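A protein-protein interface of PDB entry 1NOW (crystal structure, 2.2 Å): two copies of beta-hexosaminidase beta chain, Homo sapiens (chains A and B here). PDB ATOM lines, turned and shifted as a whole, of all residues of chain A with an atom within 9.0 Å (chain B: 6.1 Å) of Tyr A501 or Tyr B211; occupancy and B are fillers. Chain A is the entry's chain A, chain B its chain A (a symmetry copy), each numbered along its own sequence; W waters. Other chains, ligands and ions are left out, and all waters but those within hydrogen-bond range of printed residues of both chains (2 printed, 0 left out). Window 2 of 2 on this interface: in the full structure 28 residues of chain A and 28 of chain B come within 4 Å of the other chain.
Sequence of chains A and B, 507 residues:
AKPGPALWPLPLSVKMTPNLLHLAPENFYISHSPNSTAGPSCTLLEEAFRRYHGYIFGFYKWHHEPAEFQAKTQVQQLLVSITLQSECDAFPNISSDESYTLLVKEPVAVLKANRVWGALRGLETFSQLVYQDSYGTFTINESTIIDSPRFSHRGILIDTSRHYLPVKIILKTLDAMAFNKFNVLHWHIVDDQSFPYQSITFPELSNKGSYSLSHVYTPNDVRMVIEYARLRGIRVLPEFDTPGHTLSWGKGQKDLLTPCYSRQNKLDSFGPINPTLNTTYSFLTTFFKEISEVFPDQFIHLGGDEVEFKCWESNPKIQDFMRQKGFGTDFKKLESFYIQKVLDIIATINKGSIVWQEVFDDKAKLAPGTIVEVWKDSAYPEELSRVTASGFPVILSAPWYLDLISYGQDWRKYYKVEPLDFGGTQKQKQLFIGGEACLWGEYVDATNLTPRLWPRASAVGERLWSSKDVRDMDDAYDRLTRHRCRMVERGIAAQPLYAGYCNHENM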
ATOM      1  N   TYR A 477      22.198  23.197 -10.620  1.00  0.00           N
ATOM      2  CA  TYR A 477      21.823  21.935  -9.998  1.00  0.00           C
ATOM      3  C   TYR A 477      21.949  20.792 -10.997  1.00  0.00           C
ATOM      4  O   TYR A 477      22.468  19.744 -10.652  1.00  0.00           O
ATOM      5  CB  TYR A 477      20.400  22.000  -9.464  1.00  0.00           C
ATOM      6  CG  TYR A 477      19.868  20.702  -8.890  1.00  0.00           C
ATOM      7  CD1 TYR A 477      20.193  20.311  -7.604  1.00  0.00           C
ATOM      8  CD2 TYR A 477      19.017  19.890  -9.623  1.00  0.00           C
ATOM      9  CE1 TYR A 477      19.697  19.145  -7.058  1.00  0.00           C
ATOM     10  CE2 TYR A 477      18.510  18.706  -9.085  1.00  0.00           C
ATOM     11  CZ  TYR A 477      18.871  18.340  -7.803  1.00  0.00           C
ATOM     12  OH  TYR A 477      18.392  17.188  -7.237  1.00  0.00           O
ATOM     13  N   THR A 481      24.853  17.937 -10.060  1.00  0.00           N
ATOM     14  CA  THR A 481      24.507  16.561  -9.692  1.00  0.00           C
ATOM     15  C   THR A 481      25.273  15.563 -10.572  1.00  0.00           C
ATOM     16  O   THR A 481      25.700  14.525 -10.090  1.00  0.00           O
ATOM     17  CB  THR A 481      22.998  16.256  -9.843  1.00  0.00           C
ATOM     18  OG1 THR A 481      22.536  16.699 -11.115  1.00  0.00           O
ATOM     19  CG2 THR A 481      22.146  17.001  -8.836  1.00  0.00           C
ATOM     20  N   ARG A 482      25.441  15.884 -11.858  1.00  0.00           N
ATOM     21  CA  ARG A 482      26.169  15.003 -12.781  1.00  0.00           C
ATOM     22  C   ARG A 482      27.682  15.074 -12.543  1.00  0.00           C
ATOM     23  O   ARG A 482      28.355  14.044 -12.568  1.00  0.00           O
ATOM     24  CB  ARG A 482      25.811  15.326 -14.230  1.00  0.00           C
ATOM     25  CG  ARG A 482      24.351  15.002 -14.560  1.00  0.00           C
ATOM     26  CD  ARG A 482      23.745  15.884 -15.635  1.00  0.00           C
ATOM     27  NE  ARG A 482      24.110  15.460 -16.988  1.00  0.00           N
ATOM     28  CZ  ARG A 482      24.146  16.248 -18.081  1.00  0.00           C
ATOM     29  NH1 ARG A 482      23.864  17.563 -18.035  1.00  0.00           N
ATOM     30  NH2 ARG A 482      24.497  15.706 -19.248  1.00  0.00           N
ATOM     31  N   ARG A 484      29.037  15.772  -9.699  1.00  0.00           N
ATOM     32  CA  ARG A 484      29.200  15.015  -8.467  1.00  0.00           C
ATOM     33  C   ARG A 484      29.239  13.506  -8.727  1.00  0.00           C
ATOM     34  O   ARG A 484      30.044  12.810  -8.131  1.00  0.00           O
ATOM     35  CB  ARG A 484      28.087  15.398  -7.488  1.00  0.00           C
ATOM     36  CG  ARG A 484      28.111  14.678  -6.201  1.00  0.00           C
ATOM     37  CD  ARG A 484      27.114  13.578  -6.146  1.00  0.00           C
ATOM     38  NE  ARG A 484      27.359  12.672  -5.040  1.00  0.00           N
ATOM     39  CZ  ARG A 484      26.585  11.652  -4.722  1.00  0.00           C
ATOM     40  NH1 ARG A 484      25.486  11.380  -5.421  1.00  0.00           N
ATOM     41  NH2 ARG A 484      26.920  10.891  -3.692  1.00  0.00           N
ATOM     42  N   CYS A 485      28.373  13.004  -9.605  1.00  0.00           N
ATOM     43  CA  CYS A 485      28.407  11.584  -9.981  1.00  0.00           C
ATOM     44  C   CYS A 485      29.732  11.229 -10.657  1.00  0.00           C
ATOM     45  O   CYS A 485      30.270  10.146 -10.446  1.00  0.00           O
ATOM     46  CB  CYS A 485      27.242  11.208 -10.903  1.00  0.00           C
ATOM     47  SG  CYS A 485      25.658  11.109 -10.045  1.00  0.00           S
ATOM     48  N   VAL A 488      32.355  10.779  -7.976  1.00  0.00           N
ATOM     49  CA  VAL A 488      32.193   9.463  -7.379  1.00  0.00           C
ATOM     50  C   VAL A 488      32.797   8.383  -8.276  1.00  0.00           C
ATOM     51  O   VAL A 488      33.564   7.567  -7.779  1.00  0.00           O
ATOM     52  CB  VAL A 488      30.721   9.185  -7.002  1.00  0.00           C
ATOM     53  CG1 VAL A 488      30.514   7.733  -6.535  1.00  0.00           C
ATOM     54  CG2 VAL A 488      30.294  10.140  -5.877  1.00  0.00           C
ATOM     55  N   GLU A 489      32.508   8.423  -9.580  1.00  0.00           N
ATOM     56  CA  GLU A 489      33.080   7.478 -10.551  1.00  0.00           C
ATOM     57  C   GLU A 489      34.611   7.477 -10.553  1.00  0.00           C
ATOM     58  O   GLU A 489      35.230   6.444 -10.780  1.00  0.00           O
ATOM     59  CB  GLU A 489      32.618   7.797 -11.970  1.00  0.00           C
ATOM     60  CG  GLU A 489      31.148   7.521 -12.252  1.00  0.00           C
ATOM     61  CD  GLU A 489      30.620   8.237 -13.498  1.00  0.00           C
ATOM     62  OE1 GLU A 489      31.435   8.681 -14.350  1.00  0.00           O
ATOM     63  OE2 GLU A 489      29.376   8.351 -13.639  1.00  0.00           O
ATOM     64  N   PRO A 496      25.769  13.613  -1.764  1.00  0.00           N
ATOM     65  CA  PRO A 496      24.664  14.039  -2.624  1.00  0.00           C
ATOM     66  C   PRO A 496      24.274  15.500  -2.476  1.00  0.00           C
ATOM     67  O   PRO A 496      24.548  16.106  -1.449  1.00  0.00           O
ATOM     68  CB  PRO A 496      23.486  13.194  -2.143  1.00  0.00           C
ATOM     69  CG  PRO A 496      24.065  12.138  -1.318  1.00  0.00           C
ATOM     70  CD  PRO A 496      25.308  12.651  -0.748  1.00  0.00           C
ATOM     71  N   LEU A 497      23.645  16.043  -3.512  1.00  0.00           N
ATOM     72  CA  LEU A 497      23.046  17.371  -3.438  1.00  0.00           C
ATOM     73  C   LEU A 497      21.635  17.248  -2.892  1.00  0.00           C
ATOM     74  O   LEU A 497      21.180  18.134  -2.188  1.00  0.00           O
ATOM     75  CB  LEU A 497      22.987  18.064  -4.803  1.00  0.00           C
ATOM     76  CG  LEU A 497      24.262  18.575  -5.477  1.00  0.00           C
ATOM     77  CD1 LEU A 497      23.900  19.455  -6.644  1.00  0.00           C
ATOM     78  CD2 LEU A 497      25.163  19.367  -4.563  1.00  0.00           C
ATOM     79  N   TYR A 498      20.943  16.171  -3.253  1.00  0.00           N
ATOM     80  CA  TYR A 498      19.561  15.944  -2.885  1.00  0.00           C
ATOM     81  C   TYR A 498      19.266  14.472  -3.221  1.00  0.00           C
ATOM     82  O   TYR A 498      20.191  13.720  -3.576  1.00  0.00           O
ATOM     83  CB  TYR A 498      18.624  16.927  -3.631  1.00  0.00           C
ATOM     84  CG  TYR A 498      17.192  16.962  -3.114  1.00  0.00           C
ATOM     85  CD1 TYR A 498      16.924  17.223  -1.780  1.00  0.00           C
ATOM     86  CD2 TYR A 498      16.121  16.643  -3.943  1.00  0.00           C
ATOM     87  CE1 TYR A 498      15.641  17.219  -1.289  1.00  0.00           C
ATOM     88  CE2 TYR A 498      14.830  16.632  -3.462  1.00  0.00           C
ATOM     89  CZ  TYR A 498      14.597  16.924  -2.128  1.00  0.00           C
ATOM     90  OH  TYR A 498      13.309  16.909  -1.631  1.00  0.00           O
ATOM     91  N   ALA A 499      18.024  14.031  -3.025  1.00  0.00           N
ATOM     92  CA  ALA A 499      17.602  12.678  -3.369  1.00  0.00           C
ATOM     93  C   ALA A 499      17.928  12.367  -4.819  1.00  0.00           C
ATOM     94  O   ALA A 499      17.973  13.265  -5.657  1.00  0.00           O
ATOM     95  CB  ALA A 499      16.110  12.509  -3.133  1.00  0.00           C
ATOM     96  N   GLY A 500      18.161  11.091  -5.104  1.00  0.00           N
ATOM     97  CA  GLY A 500      18.502  10.660  -6.444  1.00  0.00           C
ATOM     98  C   GLY A 500      19.458   9.497  -6.443  1.00  0.00           C
ATOM     99  O   GLY A 500      19.599   8.780  -5.454  1.00  0.00           O
ATOM    100  N   TYR A 501      20.096   9.286  -7.580  1.00  0.00           N
ATOM    101  CA  TYR A 501      21.057   8.218  -7.742  1.00  0.00           C
ATOM    102  C   TYR A 501      22.004   8.573  -8.873  1.00  0.00           C
ATOM    103  O   TYR A 501      21.733   9.480  -9.654  1.00  0.00           O
ATOM    104  CB  TYR A 501      20.361   6.895  -8.053  1.00  0.00           C
ATOM    105  CG  TYR A 501      19.761   6.804  -9.452  1.00  0.00           C
ATOM    106  CD1 TYR A 501      18.621   7.517  -9.795  1.00  0.00           C
ATOM    107  CD2 TYR A 501      20.321   5.971 -10.411  1.00  0.00           C
ATOM    108  CE1 TYR A 501      18.065   7.404 -11.054  1.00  0.00           C
ATOM    109  CE2 TYR A 501      19.777   5.850 -11.659  1.00  0.00           C
ATOM    110  CZ  TYR A 501      18.654   6.565 -11.983  1.00  0.00           C
ATOM    111  OH  TYR A 501      18.133   6.439 -13.248  1.00  0.00           O
ATOM    112  N   CYS A 502      23.129   7.871  -8.902  1.00  0.00           N
ATOM    113  CA  CYS A 502      24.111   7.983  -9.961  1.00  0.00           C
ATOM    114  C   CYS A 502      24.031   6.732 -10.832  1.00  0.00           C
ATOM    115  O   CYS A 502      23.628   5.680 -10.353  1.00  0.00           O
ATOM    116  CB  CYS A 502      25.510   8.109  -9.369  1.00  0.00           C
ATOM    117  SG  CYS A 502      25.809   9.693  -8.578  1.00  0.00           S
ATOM    118  N   ASN A 503      24.430   6.883 -12.093  1.00  0.00           N
ATOM    119  CA  ASN A 503      24.547   5.838 -13.138  1.00  0.00           C
ATOM    120  C   ASN A 503      23.349   5.867 -14.071  1.00  0.00           C
ATOM    121  O   ASN A 503      23.387   6.542 -15.096  1.00  0.00           O
ATOM    122  CB  ASN A 503      24.833   4.400 -12.627  1.00  0.00           C
ATOM    123  CG  ASN A 503      26.049   4.323 -11.698  1.00  0.00           C
ATOM    124  OD1 ASN A 503      27.064   4.990 -11.921  1.00  0.00           O
ATOM    125  ND2 ASN A 503      25.927   3.536 -10.623  1.00  0.00           N
ATOM    126  N   THR B 160      16.106   4.293   2.926  1.00  0.00           N
ATOM    127  CA  THR B 160      16.642   3.745   1.686  1.00  0.00           C
ATOM    128  C   THR B 160      15.844   4.104   0.433  1.00  0.00           C
ATOM    129  O   THR B 160      16.017   3.467  -0.594  1.00  0.00           O
ATOM    130  CB  THR B 160      16.800   2.234   1.763  1.00  0.00           C
ATOM    131  OG1 THR B 160      15.528   1.619   2.011  1.00  0.00           O
ATOM    132  CG2 THR B 160      17.707   1.859   2.901  1.00  0.00           C
ATOM    133  N   SER B 161      15.000   5.127   0.509  1.00  0.00           N
ATOM    134  CA  SER B 161      14.221   5.606  -0.636  1.00  0.00           C
ATOM    135  C   SER B 161      14.824   6.890  -1.212  1.00  0.00           C
ATOM    136  O   SER B 161      14.993   7.019  -2.435  1.00  0.00           O
ATOM    137  CB  SER B 161      12.774   5.869  -0.230  1.00  0.00           C
ATOM    138  OG  SER B 161      12.031   6.406  -1.317  1.00  0.00           O
ATOM    139  N   ARG B 162      15.113   7.854  -0.341  1.00  0.00           N
ATOM    140  CA  ARG B 162      15.699   9.118  -0.787  1.00  0.00           C
ATOM    141  C   ARG B 162      17.044   8.842  -1.472  1.00  0.00           C
ATOM    142  O   ARG B 162      17.405   9.495  -2.449  1.00  0.00           O
ATOM    143  CB  ARG B 162      15.814  10.112   0.352  1.00  0.00           C
ATOM    144  CG  ARG B 162      14.501  10.867   0.673  1.00  0.00           C
ATOM    145  CD  ARG B 162      13.238   9.999   0.807  1.00  0.00           C
ATOM    146  NE  ARG B 162      12.081  10.813   1.143  1.00  0.00           N
ATOM    147  CZ  ARG B 162      11.714  11.212   2.370  1.00  0.00           C
ATOM    148  NH1 ARG B 162      12.399  10.867   3.470  1.00  0.00           N
ATOM    149  NH2 ARG B 162      10.625  11.976   2.503  1.00  0.00           N
ATOM    150  N   HIS B 163      17.754   7.844  -0.961  1.00  0.00           N
ATOM    151  CA  HIS B 163      18.902   7.268  -1.647  1.00  0.00           C
ATOM    152  C   HIS B 163      18.887   5.792  -1.334  1.00  0.00           C
ATOM    153  O   HIS B 163      18.539   5.411  -0.214  1.00  0.00           O
ATOM    154  CB  HIS B 163      20.181   7.861  -1.127  1.00  0.00           C
ATOM    155  CG  HIS B 163      20.378   9.284  -1.522  1.00  0.00           C
ATOM    156  ND1 HIS B 163      20.712  10.267  -0.630  1.00  0.00           N
ATOM    157  CD2 HIS B 163      20.276   9.890  -2.718  1.00  0.00           C
ATOM    158  CE1 HIS B 163      20.817  11.418  -1.266  1.00  0.00           C
ATOM    159  NE2 HIS B 163      20.555  11.215  -2.536  1.00  0.00           N
ATOM    160  N   TYR B 164      19.215   4.968  -2.315  1.00  0.00           N
ATOM    161  CA  TYR B 164      19.369   3.549  -2.086  1.00  0.00           C
ATOM    162  C   TYR B 164      20.640   3.357  -1.252  1.00  0.00           C
ATOM    163  O   TYR B 164      21.600   4.038  -1.488  1.00  0.00           O
ATOM    164  CB  TYR B 164      19.559   2.845  -3.422  1.00  0.00           C
ATOM    165  CG  TYR B 164      19.775   1.352  -3.330  1.00  0.00           C
ATOM    166  CD1 TYR B 164      18.707   0.484  -3.149  1.00  0.00           C
ATOM    167  CD2 TYR B 164      21.045   0.808  -3.454  1.00  0.00           C
ATOM    168  CE1 TYR B 164      18.901  -0.885  -3.088  1.00  0.00           C
ATOM    169  CE2 TYR B 164      21.246  -0.564  -3.400  1.00  0.00           C
ATOM    170  CZ  TYR B 164      20.170  -1.399  -3.212  1.00  0.00           C
ATOM    171  OH  TYR B 164      20.366  -2.754  -3.147  1.00  0.00           O
ATOM    172  N   GLN B 193      10.445   9.164  -3.659  1.00  0.00           N
ATOM    173  CA  GLN B 193      11.460   9.171  -4.690  1.00  0.00           C
ATOM    174  C   GLN B 193      11.780   7.803  -5.286  1.00  0.00           C
ATOM    175  O   GLN B 193      12.109   7.724  -6.473  1.00  0.00           O
ATOM    176  CB  GLN B 193      12.725   9.888  -4.201  1.00  0.00           C
ATOM    177  CG  GLN B 193      12.547  11.410  -3.945  1.00  0.00           C
ATOM    178  CD  GLN B 193      12.107  11.776  -2.523  1.00  0.00           C
ATOM    179  OE1 GLN B 193      11.613  10.932  -1.765  1.00  0.00           O
ATOM    180  NE2 GLN B 193      12.291  13.042  -2.159  1.00  0.00           N
ATOM    181  N   SER B 194      11.664   6.735  -4.501  1.00  0.00           N
ATOM    182  CA  SER B 194      11.920   5.394  -5.030  1.00  0.00           C
ATOM    183  C   SER B 194      11.284   4.311  -4.180  1.00  0.00           C
ATOM    184  O   SER B 194      10.984   4.527  -3.000  1.00  0.00           O
ATOM    185  CB  SER B 194      13.424   5.126  -5.175  1.00  0.00           C
ATOM    186  OG  SER B 194      14.066   5.120  -3.917  1.00  0.00           O
ATOM    187  N   PHE B 195      11.087   3.157  -4.814  1.00  0.00           N
ATOM    188  CA  PHE B 195      10.505   1.967  -4.215  1.00  0.00           C
ATOM    189  C   PHE B 195      11.472   0.784  -4.438  1.00  0.00           C
ATOM    190  O   PHE B 195      11.298   0.005  -5.365  1.00  0.00           O
ATOM    191  CB  PHE B 195       9.134   1.666  -4.841  1.00  0.00           C
ATOM    192  CG  PHE B 195       8.272   0.760  -4.001  1.00  0.00           C
ATOM    193  CD1 PHE B 195       8.470  -0.614  -3.981  1.00  0.00           C
ATOM    194  CD2 PHE B 195       7.261   1.284  -3.218  1.00  0.00           C
ATOM    195  CE1 PHE B 195       7.671  -1.419  -3.200  1.00  0.00           C
ATOM    196  CE2 PHE B 195       6.478   0.463  -2.449  1.00  0.00           C
ATOM    197  CZ  PHE B 195       6.682  -0.872  -2.439  1.00  0.00           C
ATOM    198  N   PRO B 196      12.528   0.673  -3.643  1.00  0.00           N
ATOM    199  CA  PRO B 196      13.467  -0.455  -3.798  1.00  0.00           C
ATOM    200  C   PRO B 196      12.988  -1.812  -3.227  1.00  0.00           C
ATOM    201  O   PRO B 196      13.619  -2.816  -3.517  1.00  0.00           O
ATOM    202  CB  PRO B 196      14.696   0.022  -3.043  1.00  0.00           C
ATOM    203  CG  PRO B 196      14.162   0.924  -2.005  1.00  0.00           C
ATOM    204  CD  PRO B 196      12.975   1.624  -2.615  1.00  0.00           C
ATOM    205  N   SER B 206       8.512  -2.553  -7.476  1.00  0.00           N
ATOM    206  CA  SER B 206       9.934  -2.273  -7.614  1.00  0.00           C
ATOM    207  C   SER B 206      10.377  -2.132  -9.080  1.00  0.00           C
ATOM    208  O   SER B 206      11.182  -1.242  -9.391  1.00  0.00           O
ATOM    209  CB  SER B 206      10.791  -3.308  -6.892  1.00  0.00           C
ATOM    210  OG  SER B 206      10.689  -4.593  -7.482  1.00  0.00           O
ATOM    211  N   GLY B 209       9.094   1.319  -9.849  1.00  0.00           N
ATOM    212  CA  GLY B 209       9.330   2.331  -8.831  1.00  0.00           C
ATOM    213  C   GLY B 209      10.752   2.484  -8.319  1.00  0.00           C
ATOM    214  O   GLY B 209      11.043   3.464  -7.638  1.00  0.00           O
ATOM    215  N   SER B 210      11.638   1.532  -8.607  1.00  0.00           N
ATOM    216  CA  SER B 210      13.018   1.638  -8.149  1.00  0.00           C
ATOM    217  C   SER B 210      13.765   2.667  -8.990  1.00  0.00           C
ATOM    218  O   SER B 210      13.305   3.054 -10.059  1.00  0.00           O
ATOM    219  CB  SER B 210      13.726   0.282  -8.231  1.00  0.00           C
ATOM    220  OG  SER B 210      13.822  -0.170  -9.568  1.00  0.00           O
ATOM    221  N   TYR B 211      14.889   3.144  -8.470  1.00  0.00           N
ATOM    222  CA  TYR B 211      15.749   4.056  -9.212  1.00  0.00           C
ATOM    223  C   TYR B 211      16.297   3.355 -10.447  1.00  0.00           C
ATOM    224  O   TYR B 211      16.428   3.954 -11.502  1.00  0.00           O
ATOM    225  CB  TYR B 211      16.917   4.530  -8.347  1.00  0.00           C
ATOM    226  CG  TYR B 211      16.610   5.684  -7.417  1.00  0.00           C
ATOM    227  CD1 TYR B 211      15.978   6.836  -7.881  1.00  0.00           C
ATOM    228  CD2 TYR B 211      16.972   5.628  -6.077  1.00  0.00           C
ATOM    229  CE1 TYR B 211      15.716   7.897  -7.040  1.00  0.00           C
ATOM    230  CE2 TYR B 211      16.721   6.683  -5.227  1.00  0.00           C
ATOM    231  CZ  TYR B 211      16.099   7.816  -5.713  1.00  0.00           C
ATOM    232  OH  TYR B 211      15.865   8.867  -4.868  1.00  0.00           O
ATOM    233  N   SER B 212      16.629   2.081 -10.293  1.00  0.00           N
ATOM    234  CA  SER B 212      17.045   1.240 -11.394  1.00  0.00           C
ATOM    235  C   SER B 212      16.912  -0.175 -10.861  1.00  0.00           C
ATOM    236  O   SER B 212      16.661  -0.372  -9.669  1.00  0.00           O
ATOM    237  CB  SER B 212      18.486   1.512 -11.811  1.00  0.00           C
ATOM    238  OG  SER B 212      19.357   0.643 -11.124  1.00  0.00           O
ATOM    239  N   LEU B 213      17.104  -1.153 -11.734  1.00  0.00           N
ATOM    240  CA  LEU B 213      16.916  -2.551 -11.350  1.00  0.00           C
ATOM    241  C   LEU B 213      18.014  -3.078 -10.448  1.00  0.00           C
ATOM    242  O   LEU B 213      17.804  -4.067  -9.761  1.00  0.00           O
ATOM    243  CB  LEU B 213      16.693  -3.454 -12.568  1.00  0.00           C
ATOM    244  CG  LEU B 213      15.203  -3.680 -12.865  1.00  0.00           C
ATOM    245  CD1 LEU B 213      14.496  -2.397 -13.331  1.00  0.00           C
ATOM    246  CD2 LEU B 213      15.078  -4.762 -13.892  1.00  0.00           C
ATOM    247  N   HIS B 215      19.055  -1.115  -7.978  1.00  0.00           N
ATOM    248  CA  HIS B 215      18.820  -0.383  -6.733  1.00  0.00           C
ATOM    249  C   HIS B 215      17.535  -0.981  -6.140  1.00  0.00           C
ATOM    250  O   HIS B 215      16.515  -0.309  -6.017  1.00  0.00           O
ATOM    251  CB  HIS B 215      18.650   1.120  -6.997  1.00  0.00           C
ATOM    252  CG  HIS B 215      19.881   1.796  -7.522  1.00  0.00           C
ATOM    253  ND1 HIS B 215      20.326   1.636  -8.819  1.00  0.00           N
ATOM    254  CD2 HIS B 215      20.745   2.658  -6.932  1.00  0.00           C
ATOM    255  CE1 HIS B 215      21.422   2.354  -8.995  1.00  0.00           C
ATOM    256  NE2 HIS B 215      21.702   2.976  -7.864  1.00  0.00           N
HETATM  257  O   HOH W   1      21.781  11.741  -5.265  1.00  0.00           O
HETATM  258  O   HOH W   2      20.451   6.298  -4.547  1.00  0.00           O
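Among the printed residues, merely in contact across the chains: Pro A496 with His B163 (3.3 Å), Ala A499 with Arg B162 (3.3 Å), Ala A499 with His B163 (3.4 Å), Ala A499 with Gln B193 (3.8 Å) and Gly A500 with His B163 (3.0 Å).
Tyr A501 touches one residue of chain B. Tyr B211 touches just these residues of chain A: Gly A500 and Tyr A501. Ser B210 touches none of the printed residues of chain A. No residue of chain A comes within 4 Å of Ser B212. Printed residues of chain A within 4 Å of Arg B162: Ala A499 and Gly A500. Of the printed residues of chain B, Pro A496 touches His B163. Printed residues of chain B within 4 Å of Gly A500: Arg B162, His B163 and Tyr B211. The nearest residue of chain A that does not touch Tyr B211 is Ala A499 (4.04 Å). The nearest printed residue of chain A that does not touch Gln B193 is Tyr A498 (4.03 Å).
Of the 15 printed residues of chain A, 5 touch a printed residue of chain B. Hydrophobic or aromatic side chains of chain A that line the printed part of chain B: Pro A496, Ala A499 and Tyr A501. Hydrophobic or aromatic side chains of chain B that line the printed part of chain A: His B163 and Tyr B211. Among the printed residues, 9 pairs touch across the chains. Among the printed residues, no Asp or Glu carboxylate lies within 4 Å of a Lys or Arg side-chain nitrogen of the other chain.
The backbone carbonyl oxygen of Tyr A498 sits at hydrogen-bond distance from a ring nitrogen (NE2) of His B163 (2.7 Å). N of Gly A500 sits at hydrogen-bond distance from O of Arg B162. OH of Tyr A501 lies close to O of Tyr B211 (3.5 Å). N of Gly A500 sits at hydrogen-bond distance from OH of Tyr B211 (3.2 Å).
The side-chain hydroxyl of Tyr B211 is in hydrogen-bond range of the backbone carbonyl oxygen of Arg B162 (2.9 Å). The side-chain sulfur (SG) of Cys A485 is disulfide-bonded to the side-chain sulfur (SG) of Cys A502, at 2.0 Å. O of Ser B161 sits at hydrogen-bond distance from OH of Tyr B211, at 3.2 Å. NE of Arg B162 sits at hydrogen-bond distance from OE1 of Gln B193 (2.9 Å).
Water W2 bridges the backbone carbonyl oxygen (O) of Gly A500 (2.8 Å) and the backbone NH (N) of Tyr B164 (2.9 Å). Water W1 bridges a ring nitrogen (NE2) of His B163 and the backbone carbonyl oxygen of Tyr A498.
No position is printed for both chains. Of the 9 pairs that touch across the chains among the printed residues, none has its exchanged pair printed and touching as well.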
